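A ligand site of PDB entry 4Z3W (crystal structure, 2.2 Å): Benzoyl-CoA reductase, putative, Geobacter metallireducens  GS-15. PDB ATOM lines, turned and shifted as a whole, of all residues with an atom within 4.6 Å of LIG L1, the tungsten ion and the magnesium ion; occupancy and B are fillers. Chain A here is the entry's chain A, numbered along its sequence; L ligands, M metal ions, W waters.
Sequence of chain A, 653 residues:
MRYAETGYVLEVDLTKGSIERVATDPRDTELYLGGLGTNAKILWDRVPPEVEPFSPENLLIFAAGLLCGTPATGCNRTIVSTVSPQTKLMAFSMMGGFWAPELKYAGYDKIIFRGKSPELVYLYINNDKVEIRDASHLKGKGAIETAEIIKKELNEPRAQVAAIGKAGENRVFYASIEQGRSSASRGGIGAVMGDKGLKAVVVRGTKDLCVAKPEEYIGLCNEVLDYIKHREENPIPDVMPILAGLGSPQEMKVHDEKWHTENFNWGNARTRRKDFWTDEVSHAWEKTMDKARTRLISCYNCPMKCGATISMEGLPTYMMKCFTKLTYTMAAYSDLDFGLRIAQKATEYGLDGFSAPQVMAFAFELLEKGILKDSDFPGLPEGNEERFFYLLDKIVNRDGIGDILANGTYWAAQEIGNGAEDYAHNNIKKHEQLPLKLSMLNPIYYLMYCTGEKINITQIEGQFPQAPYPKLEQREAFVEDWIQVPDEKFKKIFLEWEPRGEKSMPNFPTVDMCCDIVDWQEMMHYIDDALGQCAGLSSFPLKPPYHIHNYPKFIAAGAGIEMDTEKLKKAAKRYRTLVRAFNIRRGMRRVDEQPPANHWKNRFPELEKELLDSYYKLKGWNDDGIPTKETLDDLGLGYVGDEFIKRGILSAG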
ATOM      1  N   ARG A  77     -32.507 -29.646 -11.134  1.00  0.00           N
ATOM      2  CA  ARG A  77     -31.613 -30.612 -11.759  1.00  0.00           C
ATOM      3  C   ARG A  77     -32.128 -32.043 -11.783  1.00  0.00           C
ATOM      4  O   ARG A  77     -32.691 -32.560 -10.805  1.00  0.00           O
ATOM      5  CB  ARG A  77     -30.237 -30.585 -11.060  1.00  0.00           C
ATOM      6  CG  ARG A  77     -29.131 -29.948 -11.919  1.00  0.00           C
ATOM      7  CD  ARG A  77     -29.394 -28.461 -12.220  1.00  0.00           C
ATOM      8  NE  ARG A  77     -28.500 -27.982 -13.275  1.00  0.00           N
ATOM      9  CZ  ARG A  77     -28.615 -26.823 -13.928  1.00  0.00           C
ATOM     10  NH1 ARG A  77     -29.605 -25.964 -13.640  1.00  0.00           N
ATOM     11  NH2 ARG A  77     -27.743 -26.520 -14.878  1.00  0.00           N
ATOM     12  N   MET A  94     -25.721 -34.797 -14.550  1.00  0.00           N
ATOM     13  CA  MET A  94     -26.744 -33.835 -14.194  1.00  0.00           C
ATOM     14  C   MET A  94     -27.229 -33.056 -15.396  1.00  0.00           C
ATOM     15  O   MET A  94     -26.451 -32.739 -16.308  1.00  0.00           O
ATOM     16  CB  MET A  94     -26.253 -32.868 -13.120  1.00  0.00           C
ATOM     17  CG  MET A  94     -26.491 -33.366 -11.701  1.00  0.00           C
ATOM     18  SD  MET A  94     -25.404 -34.769 -11.298  1.00  0.00           S
ATOM     19  CE  MET A  94     -23.859 -34.160 -11.940  1.00  0.00           C
ATOM     20  N   MET A  95     -28.522 -32.715 -15.368  1.00  0.00           N
ATOM     21  CA  MET A  95     -29.195 -32.015 -16.453  1.00  0.00           C
ATOM     22  C   MET A  95     -30.084 -30.907 -15.881  1.00  0.00           C
ATOM     23  O   MET A  95     -30.882 -31.145 -14.988  1.00  0.00           O
ATOM     24  CB  MET A  95     -30.035 -33.010 -17.281  1.00  0.00           C
ATOM     25  CG  MET A  95     -31.011 -32.392 -18.255  1.00  0.00           C
ATOM     26  SD  MET A  95     -32.028 -33.665 -19.072  1.00  0.00           S
ATOM     27  CE  MET A  95     -30.936 -34.167 -20.383  1.00  0.00           C
ATOM     28  N   GLY A  96     -29.905 -29.677 -16.374  1.00  0.00           N
ATOM     29  CA  GLY A  96     -30.700 -28.560 -15.913  1.00  0.00           C
ATOM     30  C   GLY A  96     -32.059 -28.439 -16.609  1.00  0.00           C
ATOM     31  O   GLY A  96     -32.727 -29.427 -16.916  1.00  0.00           O
ATOM     32  N   GLY A  97     -32.486 -27.201 -16.837  1.00  0.00           N
ATOM     33  CA  GLY A  97     -33.718 -26.932 -17.569  1.00  0.00           C
ATOM     34  C   GLY A  97     -35.001 -27.065 -16.770  1.00  0.00           C
ATOM     35  O   GLY A  97     -35.168 -26.452 -15.711  1.00  0.00           O
ATOM     36  N   ARG A 181     -32.341 -26.470 -23.318  1.00  0.00           N
ATOM     37  CA  ARG A 181     -31.034 -25.832 -23.063  1.00  0.00           C
ATOM     38  C   ARG A 181     -30.214 -26.615 -22.009  1.00  0.00           C
ATOM     39  O   ARG A 181     -29.375 -26.056 -21.294  1.00  0.00           O
ATOM     40  CB  ARG A 181     -31.235 -24.369 -22.629  1.00  0.00           C
ATOM     41  CG  ARG A 181     -31.357 -24.101 -21.117  1.00  0.00           C
ATOM     42  CD  ARG A 181     -30.680 -22.775 -20.787  1.00  0.00           C
ATOM     43  NE  ARG A 181     -30.149 -22.679 -19.428  1.00  0.00           N
ATOM     44  CZ  ARG A 181     -28.969 -23.153 -19.045  1.00  0.00           C
ATOM     45  NH1 ARG A 181     -28.559 -23.029 -17.781  1.00  0.00           N
ATOM     46  NH2 ARG A 181     -28.199 -23.776 -19.911  1.00  0.00           N
ATOM     47  N   SER A 182     -30.419 -27.923 -21.956  1.00  0.00           N
ATOM     48  CA  SER A 182     -29.877 -28.757 -20.908  1.00  0.00           C
ATOM     49  C   SER A 182     -29.385 -30.091 -21.441  1.00  0.00           C
ATOM     50  O   SER A 182     -29.850 -30.552 -22.481  1.00  0.00           O
ATOM     51  CB  SER A 182     -30.925 -28.971 -19.817  1.00  0.00           C
ATOM     52  OG  SER A 182     -31.343 -27.709 -19.324  1.00  0.00           O
ATOM     53  N   SER A 183     -28.448 -30.690 -20.722  1.00  0.00           N
ATOM     54  CA  SER A 183     -27.813 -31.913 -21.184  1.00  0.00           C
ATOM     55  C   SER A 183     -27.206 -32.726 -20.041  1.00  0.00           C
ATOM     56  O   SER A 183     -26.436 -32.181 -19.252  1.00  0.00           O
ATOM     57  CB  SER A 183     -26.736 -31.577 -22.218  1.00  0.00           C
ATOM     58  OG  SER A 183     -25.959 -32.732 -22.545  1.00  0.00           O
ATOM     59  N   ALA A 184     -27.627 -33.990 -19.928  1.00  0.00           N
ATOM     60  CA  ALA A 184     -26.876 -35.009 -19.192  1.00  0.00           C
ATOM     61  C   ALA A 184     -25.823 -35.475 -20.165  1.00  0.00           C
ATOM     62  O   ALA A 184     -26.110 -36.252 -21.073  1.00  0.00           O
ATOM     63  CB  ALA A 184     -27.768 -36.180 -18.761  1.00  0.00           C
ATOM     64  N   SER A 185     -24.618 -34.967 -19.983  1.00  0.00           N
ATOM     65  CA  SER A 185     -23.612 -34.995 -21.044  1.00  0.00           C
ATOM     66  C   SER A 185     -22.595 -36.146 -21.001  1.00  0.00           C
ATOM     67  O   SER A 185     -22.208 -36.698 -22.034  1.00  0.00           O
ATOM     68  CB  SER A 185     -22.839 -33.667 -21.040  1.00  0.00           C
ATOM     69  OG  SER A 185     -23.716 -32.564 -21.167  1.00  0.00           O
ATOM     70  N   SER A 248     -23.478 -20.944 -13.789  1.00  0.00           N
ATOM     71  CA  SER A 248     -22.477 -21.693 -14.543  1.00  0.00           C
ATOM     72  C   SER A 248     -21.535 -20.677 -15.165  1.00  0.00           C
ATOM     73  O   SER A 248     -21.914 -19.513 -15.292  1.00  0.00           O
ATOM     74  CB  SER A 248     -23.119 -22.556 -15.623  1.00  0.00           C
ATOM     75  OG  SER A 248     -24.081 -23.430 -15.054  1.00  0.00           O
ATOM     76  N   PRO A 249     -20.322 -21.108 -15.554  1.00  0.00           N
ATOM     77  CA  PRO A 249     -19.392 -20.170 -16.212  1.00  0.00           C
ATOM     78  C   PRO A 249     -20.105 -19.344 -17.276  1.00  0.00           C
ATOM     79  O   PRO A 249     -20.670 -19.878 -18.216  1.00  0.00           O
ATOM     80  CB  PRO A 249     -18.347 -21.107 -16.826  1.00  0.00           C
ATOM     81  CG  PRO A 249     -18.291 -22.233 -15.827  1.00  0.00           C
ATOM     82  CD  PRO A 249     -19.707 -22.422 -15.315  1.00  0.00           C
ATOM     83  N   LYS A 321     -24.435 -23.520 -23.288  1.00  0.00           N
ATOM     84  CA  LYS A 321     -23.900 -22.810 -22.136  1.00  0.00           C
ATOM     85  C   LYS A 321     -22.470 -23.289 -21.860  1.00  0.00           C
ATOM     86  O   LYS A 321     -22.026 -24.284 -22.425  1.00  0.00           O
ATOM     87  CB  LYS A 321     -24.777 -23.027 -20.903  1.00  0.00           C
ATOM     88  CG  LYS A 321     -24.378 -24.201 -20.015  1.00  0.00           C
ATOM     89  CD  LYS A 321     -24.481 -25.541 -20.739  1.00  0.00           C
ATOM     90  CE  LYS A 321     -25.954 -25.889 -21.071  1.00  0.00           C
ATOM     91  NZ  LYS A 321     -26.083 -27.288 -21.583  1.00  0.00           N
ATOM     92  N   CYS A 322     -21.746 -22.553 -21.034  1.00  0.00           N
ATOM     93  CA  CYS A 322     -20.452 -22.998 -20.540  1.00  0.00           C
ATOM     94  C   CYS A 322     -19.442 -23.353 -21.648  1.00  0.00           C
ATOM     95  O   CYS A 322     -19.471 -22.791 -22.740  1.00  0.00           O
ATOM     96  CB  CYS A 322     -20.653 -24.196 -19.601  1.00  0.00           C
ATOM     97  SG  CYS A 322     -19.293 -24.483 -18.407  1.00  0.00           S
ATOM     98  N   THR A 458     -14.320 -29.835 -13.268  1.00  0.00           N
ATOM     99  CA  THR A 458     -15.223 -28.670 -13.113  1.00  0.00           C
ATOM    100  C   THR A 458     -16.441 -29.028 -12.279  1.00  0.00           C
ATOM    101  O   THR A 458     -17.265 -28.171 -11.977  1.00  0.00           O
ATOM    102  CB  THR A 458     -15.707 -28.088 -14.463  1.00  0.00           C
ATOM    103  OG1 THR A 458     -16.511 -29.047 -15.151  1.00  0.00           O
ATOM    104  CG2 THR A 458     -14.541 -27.677 -15.333  1.00  0.00           C
ATOM    105  N   GLN A 459     -16.546 -30.289 -11.868  1.00  0.00           N
ATOM    106  CA  GLN A 459     -17.715 -30.682 -11.094  1.00  0.00           C
ATOM    107  C   GLN A 459     -17.337 -31.169  -9.692  1.00  0.00           C
ATOM    108  O   GLN A 459     -18.099 -31.901  -9.057  1.00  0.00           O
ATOM    109  CB  GLN A 459     -18.511 -31.752 -11.866  1.00  0.00           C
ATOM    110  CG  GLN A 459     -19.176 -31.190 -13.139  1.00  0.00           C
ATOM    111  CD  GLN A 459     -19.865 -32.240 -13.988  1.00  0.00           C
ATOM    112  OE1 GLN A 459     -19.218 -32.972 -14.733  1.00  0.00           O
ATOM    113  NE2 GLN A 459     -21.184 -32.311 -13.886  1.00  0.00           N
ATOM    114  N   ASP A 528     -25.669 -30.611  -3.628  1.00  0.00           N
ATOM    115  CA  ASP A 528     -26.383 -30.101  -4.793  1.00  0.00           C
ATOM    116  C   ASP A 528     -27.048 -31.229  -5.578  1.00  0.00           C
ATOM    117  O   ASP A 528     -28.217 -31.126  -5.971  1.00  0.00           O
ATOM    118  CB  ASP A 528     -25.432 -29.325  -5.723  1.00  0.00           C
ATOM    119  CG  ASP A 528     -24.953 -28.003  -5.114  1.00  0.00           C
ATOM    120  OD1 ASP A 528     -25.468 -27.625  -4.030  1.00  0.00           O
ATOM    121  OD2 ASP A 528     -24.082 -27.347  -5.726  1.00  0.00           O
ATOM    122  N   ASP A 529     -26.304 -32.301  -5.787  1.00  0.00           N
ATOM    123  CA  ASP A 529     -26.728 -33.390  -6.659  1.00  0.00           C
ATOM    124  C   ASP A 529     -27.763 -34.321  -6.019  1.00  0.00           C
ATOM    125  O   ASP A 529     -28.290 -35.200  -6.679  1.00  0.00           O
ATOM    126  CB  ASP A 529     -25.507 -34.192  -7.104  1.00  0.00           C
ATOM    127  CG  ASP A 529     -24.585 -33.387  -7.998  1.00  0.00           C
ATOM    128  OD1 ASP A 529     -25.043 -32.392  -8.600  1.00  0.00           O
ATOM    129  OD2 ASP A 529     -23.385 -33.741  -8.093  1.00  0.00           O
ATOM    130  N   GLN A 533     -30.284 -28.983  -6.702  1.00  0.00           N
ATOM    131  CA  GLN A 533     -29.919 -27.570  -6.754  1.00  0.00           C
ATOM    132  C   GLN A 533     -28.826 -27.322  -7.771  1.00  0.00           C
ATOM    133  O   GLN A 533     -27.824 -28.051  -7.814  1.00  0.00           O
ATOM    134  CB  GLN A 533     -29.472 -27.082  -5.377  1.00  0.00           C
ATOM    135  CG  GLN A 533     -29.083 -25.623  -5.376  1.00  0.00           C
ATOM    136  CD  GLN A 533     -30.224 -24.742  -5.770  1.00  0.00           C
ATOM    137  OE1 GLN A 533     -31.338 -24.881  -5.252  1.00  0.00           O
ATOM    138  NE2 GLN A 533     -29.991 -23.845  -6.725  1.00  0.00           N
ATOM    139  N   CYS A 534     -28.985 -26.302  -8.598  1.00  0.00           N
ATOM    140  CA  CYS A 534     -27.962 -26.016  -9.590  1.00  0.00           C
ATOM    141  C   CYS A 534     -26.674 -25.540  -8.932  1.00  0.00           C
ATOM    142  O   CYS A 534     -26.679 -24.610  -8.131  1.00  0.00           O
ATOM    143  CB  CYS A 534     -28.430 -24.966 -10.600  1.00  0.00           C
ATOM    144  SG  CYS A 534     -27.165 -24.582 -11.833  1.00  0.00           S
ATOM    145  N   ALA A 535     -25.556 -26.168  -9.284  1.00  0.00           N
ATOM    146  CA  ALA A 535     -24.255 -25.795  -8.707  1.00  0.00           C
ATOM    147  C   ALA A 535     -23.934 -24.323  -8.985  1.00  0.00           C
ATOM    148  O   ALA A 535     -23.058 -23.746  -8.340  1.00  0.00           O
ATOM    149  CB  ALA A 535     -23.186 -26.690  -9.246  1.00  0.00           C
ATOM    150  N   GLY A 536     -24.666 -23.722  -9.930  1.00  0.00           N
ATOM    151  CA  GLY A 536     -24.442 -22.338 -10.337  1.00  0.00           C
ATOM    152  C   GLY A 536     -24.791 -21.344  -9.255  1.00  0.00           C
ATOM    153  O   GLY A 536     -24.350 -20.196  -9.270  1.00  0.00           O
ATOM    154  N   PHE A 540     -20.506 -24.259  -7.187  1.00  0.00           N
ATOM    155  CA  PHE A 540     -19.544 -23.871  -8.217  1.00  0.00           C
ATOM    156  C   PHE A 540     -18.907 -22.488  -7.987  1.00  0.00           C
ATOM    157  O   PHE A 540     -17.678 -22.368  -8.004  1.00  0.00           O
ATOM    158  CB  PHE A 540     -20.169 -23.942  -9.604  1.00  0.00           C
ATOM    159  CG  PHE A 540     -19.182 -23.697 -10.713  1.00  0.00           C
ATOM    160  CD1 PHE A 540     -18.906 -22.420 -11.152  1.00  0.00           C
ATOM    161  CD2 PHE A 540     -18.517 -24.767 -11.294  1.00  0.00           C
ATOM    162  CE1 PHE A 540     -17.981 -22.196 -12.170  1.00  0.00           C
ATOM    163  CE2 PHE A 540     -17.588 -24.558 -12.296  1.00  0.00           C
ATOM    164  CZ  PHE A 540     -17.320 -23.267 -12.737  1.00  0.00           C
HETATM  165  N1  LIG L   1     -25.538 -28.455 -11.011  1.00  0.00           N
HETATM  166  C1  LIG L   1     -25.326 -29.589 -10.312  1.00  0.00           C
HETATM  167  N2  LIG L   1     -26.239 -29.868  -9.263  1.00  0.00           N
HETATM  168  N3  LIG L   1     -24.266 -30.461 -10.579  1.00  0.00           N
HETATM  169  C2  LIG L   1     -23.414 -30.121 -11.622  1.00  0.00           C
HETATM  170  O1  LIG L   1     -22.459 -30.861 -11.917  1.00  0.00           O
HETATM  171  N4  LIG L   1     -22.806 -28.492 -13.465  1.00  0.00           N
HETATM  172  C3  LIG L   1     -22.803 -27.048 -13.768  1.00  0.00           C
HETATM  173  C4  LIG L   1     -24.196 -26.506 -13.860  1.00  0.00           C
HETATM  174  N5  LIG L   1     -25.017 -26.906 -12.749  1.00  0.00           N
HETATM  175  C5  LIG L   1     -23.670 -28.879 -12.375  1.00  0.00           C
HETATM  176  C6  LIG L   1     -24.694 -28.121 -12.064  1.00  0.00           C
HETATM  177  C7  LIG L   1     -22.067 -26.648 -15.038  1.00  0.00           C
HETATM  178  S1  LIG L   1     -20.312 -26.559 -14.916  1.00  0.00           S
HETATM  179  C8  LIG L   1     -22.787 -26.359 -16.204  1.00  0.00           C
HETATM  180  S2  LIG L   1     -21.944 -25.924 -17.698  1.00  0.00           S
HETATM  181  C9  LIG L   1     -24.298 -26.501 -16.215  1.00  0.00           C
HETATM  182  O2  LIG L   1     -24.768 -27.023 -15.001  1.00  0.00           O
HETATM  183  C10 LIG L   1     -24.732 -27.434 -17.315  1.00  0.00           C
HETATM  184  O3  LIG L   1     -26.132 -27.533 -17.350  1.00  0.00           O
HETATM  185  P1  LIG L   1     -26.835 -28.757 -18.061  1.00  0.00           P
HETATM  186  O4  LIG L   1     -26.447 -28.824 -19.573  1.00  0.00           O
HETATM  187  O5  LIG L   1     -28.346 -28.570 -17.920  1.00  0.00           O
HETATM  188  O6  LIG L   1     -26.394 -30.022 -17.334  1.00  0.00           O
HETATM  189  N1  LG2 L   2     -21.883 -31.890 -23.681  1.00  0.00           N
HETATM  190  C1  LG2 L   2     -23.005 -31.419 -24.328  1.00  0.00           C
HETATM  191  N2  LG2 L   2     -23.495 -32.093 -25.487  1.00  0.00           N
HETATM  192  N3  LG2 L   2     -23.680 -30.266 -23.932  1.00  0.00           N
HETATM  193  C2  LG2 L   2     -23.178 -29.624 -22.814  1.00  0.00           C
HETATM  194  O1  LG2 L   2     -23.728 -28.624 -22.385  1.00  0.00           O
HETATM  195  N4  LG2 L   2     -21.473 -29.468 -20.988  1.00  0.00           N
HETATM  196  C3  LG2 L   2     -20.050 -29.548 -20.753  1.00  0.00           C
HETATM  197  C4  LG2 L   2     -19.762 -31.018 -20.679  1.00  0.00           C
HETATM  198  N5  LG2 L   2     -20.210 -31.702 -21.886  1.00  0.00           N
HETATM  199  C5  LG2 L   2     -21.979 -30.148 -22.131  1.00  0.00           C
HETATM  200  C6  LG2 L   2     -21.385 -31.224 -22.563  1.00  0.00           C
HETATM  201  C7  LG2 L   2     -19.769 -28.831 -19.419  1.00  0.00           C
HETATM  202  S1  LG2 L   2     -19.301 -27.099 -19.465  1.00  0.00           S
HETATM  203  C8  LG2 L   2     -19.945 -29.612 -18.258  1.00  0.00           C
HETATM  204  S2  LG2 L   2     -19.732 -28.935 -16.650  1.00  0.00           S
HETATM  205  C9  LG2 L   2     -20.322 -31.112 -18.375  1.00  0.00           C
HETATM  206  O2  LG2 L   2     -20.586 -31.552 -19.679  1.00  0.00           O
HETATM  207  C10 LG2 L   2     -21.447 -31.528 -17.456  1.00  0.00           C
HETATM  208  O3  LG2 L   2     -21.489 -32.916 -17.370  1.00  0.00           O
HETATM  209  P1  LG2 L   2     -22.808 -33.742 -17.095  1.00  0.00           P
HETATM  210  O4  LG2 L   2     -22.563 -35.233 -17.361  1.00  0.00           O
HETATM  211  O5  LG2 L   2     -23.932 -33.268 -18.068  1.00  0.00           O
HETATM  212  O6  LG2 L   2     -23.212 -33.546 -15.643  1.00  0.00           O
HETATM  213  W     W M   1     -19.638 -26.569 -17.174  1.00  0.00           W
HETATM  214 MG    MG M   2     -25.167 -31.684 -17.474  1.00  0.00          MG
HETATM  215  O   HOH W   1     -26.456 -29.675 -14.846  1.00  0.00           O
HETATM  216  O   HOH W   2     -21.782 -31.508  -9.311  1.00  0.00           O
HETATM  217  O   HOH W   3     -24.279 -30.937 -15.864  1.00  0.00           O
HETATM  218  O   HOH W   4     -29.351 -26.227 -18.369  1.00  0.00           O
HETATM  219  O   HOH W   5     -20.216 -28.142 -11.241  1.00  0.00           O
HETATM  220  O   HOH W   6     -24.424 -30.903 -19.090  1.00  0.00           O
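The tungsten ion is bound by a sulfur (S1) of LIG L1, a sulfur (S1) of LG2 L2, a sulfur (S2) of LG2 L2, the side-chain sulfur of Cys 322 and a sulfur (S2) of LIG L1.
Water W6 lies within hydrogen-bond range of OG of Ser 185 (2.8 Å) and O4 of LIG L1 (2.9 Å). Water W1 lies within hydrogen-bond range of the guanidinium group of Arg 77 (3.1 Å) and an oxygen (O2) of LIG L1 (3.1 Å). Water W4 lies within hydrogen-bond range of an oxygen (O5) of LIG L1 (2.6 Å), the side-chain hydroxyl (OG) of Ser 182 (2.7 Å) and the backbone carbonyl oxygen (O) of Arg 181 (2.9 Å). Water W2 bridges an oxygen (O1) of LIG L1 (2.8 Å) and the side-chain carboxylate of Asp 529 (3.0 Å). Water W5 bridges the backbone carbonyl oxygen (O) of Thr 458 (3.0 Å) and a nitrogen (N4) of LIG L1 (3.4 Å).
Within 4 Å of the tungsten ion: Cys 322. The nearest printed residue that does not touch the tungsten ion is Thr 458 (4.5 Å).
NH1 of Arg 77 lies close to SG of Cys 534 (3.3 Å). N of Gly 536 lies close to SG of Cys 534. OG of Ser 182 sits at hydrogen-bond distance from N of Gly 97 (2.8 Å). The side-chain hydroxyl (OG) of Ser 185 is in hydrogen-bond range of the side-chain hydroxyl (OG) of Ser 183. The backbone carbonyl oxygen (O) of Asp 528 is in hydrogen-bond range of the backbone NH (N) of Gln 533 (3.1 Å). The backbone carbonyl oxygen (O) of Ala 535 sits at hydrogen-bond distance from the backbone NH (N) of Phe 540 (2.8 Å). The backbone carbonyl oxygen (O) of Gly 96 sits close to the side-chain hydroxyl (OG) of Ser 182 (3.3 Å).
The magnesium ion is bound by water W6 (1.9 Å). The magnesium ion is bound by water W3, at 2.0 Å. The backbone carbonyl oxygen (O) of Met 94 binds the magnesium ion, at 2.0 Å. The magnesium ion is bound by an oxygen (O6) of LIG L1 (2.1 Å). The magnesium ion is bound by O5 of LG2 L2, 2.1 Å away. O of Ser 183 is bound to the magnesium ion (2.2 Å).
Merely in contact with LIG L1: Ser 248, Met 95 and Asp 528. Hydrophobic or aromatic side chains within 4 Å of LIG L1: Met 94 and Ala 535. Within 4 Å of LIG L1: Arg 77, Met 94, Met 95, Gly 96, Ser 182, Ser 183, Ser 248, Lys 321, Cys 322, Gln 459, Asp 528, Asp 529, Gln 533, Cys 534 and Ala 535.
Within 4 Å of the magnesium ion: Met 94 and Ser 183.
OG of Ser 182 sits close to O5 of LIG L1 (3.4 Å). The side-chain hydroxyl (OG) of Ser 185 sits close to a nitrogen (N1) of LG2 L2, 3.2 Å away. The backbone NH (N) of Ala 535 lies within hydrogen-bond range of a nitrogen (N1) of LIG L1 (2.9 Å). An oxygen (O4) of LG2 L2 sits at hydrogen-bond distance from the backbone NH (N) of Ser 185, at 3.3 Å. The backbone NH of Met 94 is in hydrogen-bond range of an oxygen (O6) of LG2 L2, 3.0 Å away. The side-chain amino group (NZ) of Lys 321 is in hydrogen-bond range of an oxygen (O1) of LG2 L2 (2.8 Å). N of Gly 96 lies within hydrogen-bond range of O5 of LIG L1, at 2.5 Å. An oxygen (O5) of LIG L1 is in salt-bridge range of the guanidinium group (NH2) of Arg 77, 3.7 Å away. NE2 of Gln 459 is in hydrogen-bond range of O1 of LIG L1 (2.8 Å). O4 of LIG L1 lies within hydrogen-bond range of N of Ser 183 (3.0 Å). A nitrogen (N2) of LIG L1 lies within hydrogen-bond range of the backbone carbonyl oxygen of Gln 533, at 2.8 Å. The side-chain amino group (NZ) of Lys 321 lies within salt-bridge range of an oxygen (O4) of LIG L1 (2.6 Å). The side-chain hydroxyl (OG1) of Thr 458 sits close to a sulfur (S2) of LG2 L2 (3.6 Å). The side-chain amide nitrogen (NE2) of Gln 459 lies within hydrogen-bond range of an oxygen (O6) of LG2 L2, at 3.0 Å. A nitrogen (N2) of LIG L1 is in hydrogen-bond range of the side-chain carboxylate of Asp 529 (2.9 Å). N5 of LIG L1 lies close to SG of Cys 534 (3.3 Å).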
